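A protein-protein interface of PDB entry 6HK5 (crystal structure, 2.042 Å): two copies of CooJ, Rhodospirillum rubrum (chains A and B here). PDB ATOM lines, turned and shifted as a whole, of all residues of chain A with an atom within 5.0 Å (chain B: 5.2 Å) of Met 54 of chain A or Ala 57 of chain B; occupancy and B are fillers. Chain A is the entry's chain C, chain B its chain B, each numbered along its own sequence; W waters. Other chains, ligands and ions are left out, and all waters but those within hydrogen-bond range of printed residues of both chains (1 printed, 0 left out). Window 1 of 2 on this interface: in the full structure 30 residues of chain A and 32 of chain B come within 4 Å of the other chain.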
ATOM      1  N   VAL A  23       4.848   1.218  18.238  1.00  0.00           N
ATOM      2  CA  VAL A  23       3.853   0.405  17.555  1.00  0.00           C
ATOM      3  C   VAL A  23       4.386  -0.040  16.202  1.00  0.00           C
ATOM      4  O   VAL A  23       4.566  -1.233  15.938  1.00  0.00           O
ATOM      5  CB  VAL A  23       2.549   1.205  17.402  1.00  0.00           C
ATOM      6  CG1 VAL A  23       1.577   0.498  16.485  1.00  0.00           C
ATOM      7  CG2 VAL A  23       1.961   1.510  18.766  1.00  0.00           C
ATOM      8  N   HIS A  26       7.554  -2.151  16.379  1.00  0.00           N
ATOM      9  CA  HIS A  26       7.310  -3.495  16.880  1.00  0.00           C
ATOM     10  C   HIS A  26       6.659  -4.382  15.829  1.00  0.00           C
ATOM     11  O   HIS A  26       6.949  -5.585  15.750  1.00  0.00           O
ATOM     12  CB  HIS A  26       6.434  -3.419  18.123  1.00  0.00           C
ATOM     13  CG  HIS A  26       5.793  -4.714  18.480  1.00  0.00           C
ATOM     14  ND1 HIS A  26       6.411  -5.645  19.286  1.00  0.00           N
ATOM     15  CD2 HIS A  26       4.583  -5.228  18.158  1.00  0.00           C
ATOM     16  CE1 HIS A  26       5.611  -6.684  19.439  1.00  0.00           C
ATOM     17  NE2 HIS A  26       4.499  -6.460  18.760  1.00  0.00           N
ATOM     18  N   MET A  27       5.754  -3.817  15.036  1.00  0.00           N
ATOM     19  CA  MET A  27       5.193  -4.530  13.897  1.00  0.00           C
ATOM     20  C   MET A  27       6.294  -4.927  12.887  1.00  0.00           C
ATOM     21  O   MET A  27       6.260  -6.008  12.295  1.00  0.00           O
ATOM     22  CB  MET A  27       4.116  -3.680  13.233  1.00  0.00           C
ATOM     23  CG  MET A  27       2.930  -3.367  14.166  1.00  0.00           C
ATOM     24  SD  MET A  27       1.546  -2.206  13.375  1.00  0.00           S
ATOM     25  CE  MET A  27       0.815  -3.479  12.053  1.00  0.00           C
ATOM     26  N   ALA A  50      -2.417 -10.479  17.451  1.00  0.00           N
ATOM     27  CA  ALA A  50      -1.610  -9.426  18.060  1.00  0.00           C
ATOM     28  C   ALA A  50      -1.337  -8.311  17.070  1.00  0.00           C
ATOM     29  O   ALA A  50      -1.423  -7.129  17.423  1.00  0.00           O
ATOM     30  CB  ALA A  50      -0.289  -9.990  18.591  1.00  0.00           C
ATOM     31  N   LEU A  51      -0.993  -8.671  15.824  1.00  0.00           N
ATOM     32  CA  LEU A  51      -0.656  -7.671  14.816  1.00  0.00           C
ATOM     33  C   LEU A  51      -1.858  -6.820  14.459  1.00  0.00           C
ATOM     34  O   LEU A  51      -1.725  -5.608  14.268  1.00  0.00           O
ATOM     35  CB  LEU A  51      -0.105  -8.336  13.555  1.00  0.00           C
ATOM     36  CG  LEU A  51       1.349  -8.784  13.620  1.00  0.00           C
ATOM     37  CD1 LEU A  51       1.779  -9.410  12.277  1.00  0.00           C
ATOM     38  CD2 LEU A  51       2.202  -7.575  13.988  1.00  0.00           C
ATOM     39  N   ALA A  52      -3.030  -7.440  14.309  1.00  0.00           N
ATOM     40  CA  ALA A  52      -4.210  -6.642  14.012  1.00  0.00           C
ATOM     41  C   ALA A  52      -4.510  -5.682  15.158  1.00  0.00           C
ATOM     42  O   ALA A  52      -4.898  -4.534  14.924  1.00  0.00           O
ATOM     43  CB  ALA A  52      -5.409  -7.545  13.700  1.00  0.00           C
ATOM     44  N   ASP A  53      -4.325  -6.120  16.409  1.00  0.00           N
ATOM     45  CA  ASP A  53      -4.536  -5.196  17.526  1.00  0.00           C
ATOM     46  C   ASP A  53      -3.539  -4.040  17.495  1.00  0.00           C
ATOM     47  O   ASP A  53      -3.887  -2.893  17.829  1.00  0.00           O
ATOM     48  CB  ASP A  53      -4.467  -5.938  18.855  1.00  0.00           C
ATOM     49  CG  ASP A  53      -5.664  -6.865  19.068  1.00  0.00           C
ATOM     50  OD1 ASP A  53      -6.749  -6.610  18.511  1.00  0.00           O
ATOM     51  OD2 ASP A  53      -5.509  -7.864  19.781  1.00  0.00           O
ATOM     52  N   MET A  54      -2.306  -4.307  17.079  1.00  0.00           N
ATOM     53  CA  MET A  54      -1.345  -3.216  16.906  1.00  0.00           C
ATOM     54  C   MET A  54      -1.849  -2.200  15.887  1.00  0.00           C
ATOM     55  O   MET A  54      -1.761  -0.985  16.114  1.00  0.00           O
ATOM     56  CB  MET A  54       0.037  -3.728  16.467  1.00  0.00           C
ATOM     57  CG  MET A  54       0.920  -4.368  17.553  1.00  0.00           C
ATOM     58  SD  MET A  54       1.170  -3.442  19.312  1.00  0.00           S
ATOM     59  CE  MET A  54       0.914  -1.628  18.898  1.00  0.00           C
ATOM     60  N   ALA A  55      -2.396  -2.702  14.770  1.00  0.00           N
ATOM     61  CA  ALA A  55      -2.892  -1.812  13.720  1.00  0.00           C
ATOM     62  C   ALA A  55      -4.036  -0.922  14.203  1.00  0.00           C
ATOM     63  O   ALA A  55      -4.161   0.219  13.743  1.00  0.00           O
ATOM     64  CB  ALA A  55      -3.345  -2.607  12.500  1.00  0.00           C
ATOM     65  N   VAL A  56      -4.893  -1.431  15.097  1.00  0.00           N
ATOM     66  CA  VAL A  56      -5.949  -0.603  15.670  1.00  0.00           C
ATOM     67  C   VAL A  56      -5.343   0.494  16.534  1.00  0.00           C
ATOM     68  O   VAL A  56      -5.726   1.669  16.444  1.00  0.00           O
ATOM     69  CB  VAL A  56      -6.924  -1.455  16.502  1.00  0.00           C
ATOM     70  CG1 VAL A  56      -8.037  -0.555  17.071  1.00  0.00           C
ATOM     71  CG2 VAL A  56      -7.476  -2.646  15.711  1.00  0.00           C
ATOM     72  N   ALA A  57      -4.430   0.102  17.425  1.00  0.00           N
ATOM     73  CA  ALA A  57      -3.719   1.061  18.260  1.00  0.00           C
ATOM     74  C   ALA A  57      -2.974   2.072  17.405  1.00  0.00           C
ATOM     75  O   ALA A  57      -2.937   3.265  17.731  1.00  0.00           O
ATOM     76  CB  ALA A  57      -2.749   0.330  19.185  1.00  0.00           C
ATOM     77  N   ARG A  58      -2.387   1.612  16.299  1.00  0.00           N
ATOM     78  CA  ARG A  58      -1.711   2.540  15.401  1.00  0.00           C
ATOM     79  C   ARG A  58      -2.695   3.549  14.845  1.00  0.00           C
ATOM     80  O   ARG A  58      -2.387   4.741  14.755  1.00  0.00           O
ATOM     81  CB  ARG A  58      -1.026   1.786  14.263  1.00  0.00           C
ATOM     82  CG  ARG A  58      -0.570   2.698  13.127  1.00  0.00           C
ATOM     83  CD  ARG A  58       0.016   1.897  11.951  1.00  0.00           C
ATOM     84  NE  ARG A  58       0.494   2.790  10.897  1.00  0.00           N
ATOM     85  CZ  ARG A  58      -0.262   3.236   9.900  1.00  0.00           C
ATOM     86  NH1 ARG A  58      -1.547   2.873   9.827  1.00  0.00           N
ATOM     87  NH2 ARG A  58       0.259   4.050   8.984  1.00  0.00           N
ATOM     88  N   ALA A  59      -3.891   3.083  14.475  1.00  0.00           N
ATOM     89  CA  ALA A  59      -4.913   3.976  13.936  1.00  0.00           C
ATOM     90  C   ALA A  59      -5.331   5.015  14.966  1.00  0.00           C
ATOM     91  O   ALA A  59      -5.404   6.209  14.662  1.00  0.00           O
ATOM     92  CB  ALA A  59      -6.119   3.158  13.469  1.00  0.00           C
ATOM     93  N   PHE B  19       9.673  -5.578  25.679  1.00  0.00           N
ATOM     94  CA  PHE B  19       8.828  -4.614  24.982  1.00  0.00           C
ATOM     95  C   PHE B  19       7.537  -4.362  25.740  1.00  0.00           C
ATOM     96  O   PHE B  19       7.073  -3.218  25.833  1.00  0.00           O
ATOM     97  CB  PHE B  19       8.514  -5.115  23.576  1.00  0.00           C
ATOM     98  CG  PHE B  19       7.518  -4.263  22.833  1.00  0.00           C
ATOM     99  CD1 PHE B  19       7.936  -3.169  22.097  1.00  0.00           C
ATOM    100  CD2 PHE B  19       6.162  -4.553  22.872  1.00  0.00           C
ATOM    101  CE1 PHE B  19       7.016  -2.378  21.409  1.00  0.00           C
ATOM    102  CE2 PHE B  19       5.235  -3.774  22.191  1.00  0.00           C
ATOM    103  CZ  PHE B  19       5.663  -2.683  21.458  1.00  0.00           C
ATOM    104  N   ASP B  53      -6.854   0.714  23.332  1.00  0.00           N
ATOM    105  CA  ASP B  53      -6.432  -0.170  22.253  1.00  0.00           C
ATOM    106  C   ASP B  53      -5.069  -0.789  22.547  1.00  0.00           C
ATOM    107  O   ASP B  53      -4.818  -1.944  22.180  1.00  0.00           O
ATOM    108  CB  ASP B  53      -6.441   0.598  20.918  1.00  0.00           C
ATOM    109  CG  ASP B  53      -7.871   1.020  20.488  1.00  0.00           C
ATOM    110  OD1 ASP B  53      -8.834   0.488  21.073  1.00  0.00           O
ATOM    111  OD2 ASP B  53      -8.048   1.871  19.573  1.00  0.00           O
ATOM    112  N   MET B  54      -4.204  -0.078  23.264  1.00  0.00           N
ATOM    113  CA  MET B  54      -2.921  -0.644  23.668  1.00  0.00           C
ATOM    114  C   MET B  54      -3.083  -1.752  24.694  1.00  0.00           C
ATOM    115  O   MET B  54      -2.349  -2.733  24.663  1.00  0.00           O
ATOM    116  CB  MET B  54      -2.002   0.446  24.221  1.00  0.00           C
ATOM    117  CG  MET B  54      -1.174   1.111  23.150  1.00  0.00           C
ATOM    118  SD  MET B  54      -0.355  -0.239  21.967  1.00  0.00           S
ATOM    119  CE  MET B  54       0.805  -1.185  23.233  1.00  0.00           C
ATOM    120  N   ALA B  55      -4.044  -1.587  25.611  1.00  0.00           N
ATOM    121  CA  ALA B  55      -4.353  -2.660  26.549  1.00  0.00           C
ATOM    122  C   ALA B  55      -4.825  -3.923  25.825  1.00  0.00           C
ATOM    123  O   ALA B  55      -4.477  -5.047  26.216  1.00  0.00           O
ATOM    124  CB  ALA B  55      -5.407  -2.188  27.548  1.00  0.00           C
ATOM    125  N   VAL B  56      -5.632  -3.765  24.775  1.00  0.00           N
ATOM    126  CA  VAL B  56      -5.985  -4.915  23.945  1.00  0.00           C
ATOM    127  C   VAL B  56      -4.734  -5.538  23.343  1.00  0.00           C
ATOM    128  O   VAL B  56      -4.542  -6.762  23.380  1.00  0.00           O
ATOM    129  CB  VAL B  56      -6.985  -4.512  22.851  1.00  0.00           C
ATOM    130  CG1 VAL B  56      -7.465  -5.789  22.084  1.00  0.00           C
ATOM    131  CG2 VAL B  56      -8.153  -3.749  23.467  1.00  0.00           C
ATOM    132  N   ALA B  57      -3.855  -4.706  22.783  1.00  0.00           N
ATOM    133  CA  ALA B  57      -2.654  -5.261  22.176  1.00  0.00           C
ATOM    134  C   ALA B  57      -1.820  -5.995  23.219  1.00  0.00           C
ATOM    135  O   ALA B  57      -1.275  -7.068  22.942  1.00  0.00           O
ATOM    136  CB  ALA B  57      -1.854  -4.161  21.481  1.00  0.00           C
ATOM    137  N   ARG B  58      -1.769  -5.476  24.447  1.00  0.00           N
ATOM    138  CA  ARG B  58      -1.015  -6.145  25.500  1.00  0.00           C
ATOM    139  C   ARG B  58      -1.562  -7.535  25.777  1.00  0.00           C
ATOM    140  O   ARG B  58      -0.805  -8.506  25.880  1.00  0.00           O
ATOM    141  CB  ARG B  58      -1.032  -5.304  26.770  1.00  0.00           C
ATOM    142  CG  ARG B  58      -0.312  -4.011  26.599  1.00  0.00           C
ATOM    143  CD  ARG B  58      -0.553  -3.123  27.777  1.00  0.00           C
ATOM    144  NE  ARG B  58      -0.140  -3.765  29.014  1.00  0.00           N
ATOM    145  CZ  ARG B  58      -0.951  -4.014  30.035  1.00  0.00           C
ATOM    146  NH1 ARG B  58      -2.239  -3.673  29.975  1.00  0.00           N
ATOM    147  NH2 ARG B  58      -0.458  -4.595  31.120  1.00  0.00           N
ATOM    148  N   ALA B  59      -2.877  -7.643  25.944  1.00  0.00           N
ATOM    149  CA  ALA B  59      -3.498  -8.953  26.094  1.00  0.00           C
ATOM    150  C   ALA B  59      -3.095  -9.897  24.960  1.00  0.00           C
ATOM    151  O   ALA B  59      -2.655 -11.025  25.203  1.00  0.00           O
ATOM    152  CB  ALA B  59      -5.021  -8.798  26.145  1.00  0.00           C
ATOM    153  N   SER B  60      -3.217  -9.440  23.708  1.00  0.00           N
ATOM    154  CA  SER B  60      -2.978 -10.339  22.581  1.00  0.00           C
ATOM    155  C   SER B  60      -1.496 -10.655  22.410  1.00  0.00           C
ATOM    156  O   SER B  60      -1.146 -11.766  21.983  1.00  0.00           O
ATOM    157  CB  SER B  60      -3.541  -9.732  21.292  1.00  0.00           C
ATOM    158  OG  SER B  60      -2.738  -8.651  20.847  1.00  0.00           O
ATOM    159  N   LEU B  61      -0.614  -9.695  22.706  1.00  0.00           N
ATOM    160  CA  LEU B  61       0.815  -9.988  22.629  1.00  0.00           C
ATOM    161  C   LEU B  61       1.233 -10.949  23.733  1.00  0.00           C
ATOM    162  O   LEU B  61       2.093 -11.817  23.524  1.00  0.00           O
ATOM    163  CB  LEU B  61       1.631  -8.704  22.718  1.00  0.00           C
ATOM    164  CG  LEU B  61       2.021  -8.047  21.401  1.00  0.00           C
ATOM    165  CD1 LEU B  61       2.826  -6.782  21.711  1.00  0.00           C
ATOM    166  CD2 LEU B  61       2.811  -9.023  20.519  1.00  0.00           C
ATOM    167  N   ASN B  62       0.628 -10.812  24.917  1.00  0.00           N
ATOM    168  CA  ASN B  62       0.900 -11.757  25.990  1.00  0.00           C
ATOM    169  C   ASN B  62       0.528 -13.183  25.581  1.00  0.00           C
ATOM    170  O   ASN B  62       1.228 -14.133  25.929  1.00  0.00           O
ATOM    171  CB  ASN B  62       0.141 -11.341  27.248  1.00  0.00           C
ATOM    172  CG  ASN B  62       0.858 -10.250  28.030  1.00  0.00           C
ATOM    173  OD1 ASN B  62       1.754 -10.534  28.826  1.00  0.00           O
ATOM    174  ND2 ASN B  62       0.456  -8.993  27.812  1.00  0.00           N
HETATM  175  O   HOH W   1      -5.655  -2.984  19.651  1.00  0.00           O
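The side-chain hydroxyl of Ser 60 of chain B sits at hydrogen-bond distance from the side-chain carboxylate of Asp 53 of chain A, at 3.1 Å.
O of Ala 57 of chain B lies within hydrogen-bond range of OG of Ser 60 of chain B (3.0 Å).
Among the printed residues, pairs that only touch across the chains: His 26 of chain A with Phe 19 of chain B (3.5 Å), His 26 of chain A with Leu 61 of chain B (3.4 Å), Ala 50 of chain A with Ser 60 of chain B (3.1 Å), Ala 50 of chain A with Leu 61 of chain B (3.8 Å), Asp 53 of chain A with Val 56 of chain B (3.7 Å), Asp 53 of chain A with Ala 57 of chain B (3.8 Å), Met 54 of chain A with Met 54 of chain B (3.6 Å), Met 54 of chain A with Ala 57 of chain B (3.8 Å), Val 56 of chain A with Asp 53 of chain B (3.5 Å), Ala 57 of chain A with Asp 53 of chain B (3.8 Å) and Ala 57 of chain A with Met 54 of chain B (3.7 Å).
Of chain B, only Met 54 and Ala 57 come within 4 Å of Met 54 of chain A.
Printed residues of chain A within 4 Å of Ala 57 of chain B: Asp 53 and Met 54.
Printed residues of chain B within 4 Å of Ala 50 of chain A: Ser 60 (3.1 Å) and Leu 61 (3.8 Å).
Of the printed residues of chain A, Met 54 of chain B touches Met 54 (3.6 Å) and Ala 57 (3.7 Å).
Met 27 of chain A touches none of the printed residues of chain B.
The nearest residue of chain B that does not touch Met 54 of chain A is Leu 61 of chain B (4.4 Å).
The nearest printed residue of chain A that does not touch Leu 61 of chain B is Met 54 of chain A (4.4 Å).
Hydrophobic or aromatic side chains of chain A within 4 Å of the printed part of chain B: His 26, Ala 50, Met 54, Val 56 and Ala 57.
Of the 11 printed residues of chain B, 7 touch a printed residue of chain A.
Among the printed residues, no Asp or Glu carboxylate lies within 4 Å of a Lys or Arg side-chain nitrogen of the other chain.
Asp 53 of chain A touches Val 56 of chain B, and with the chains exchanged Val 56 of chain A touches Asp 53 of chain B.
Asp 53 of chain A touches Ala 57 of chain B, and with the chains exchanged Ala 57 of chain A touches Asp 53 of chain B.
Met 54 of chain B touches its own counterpart, Met 54 of chain A.
Met 54 of chain A touches Ala 57 of chain B, and with the chains exchanged Ala 57 of chain A touches Met 54 of chain B.
Water W1 bridges O of Asp 53 of chain A (2.5 Å) and O of Asp 53 of chain B (2.9 Å).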
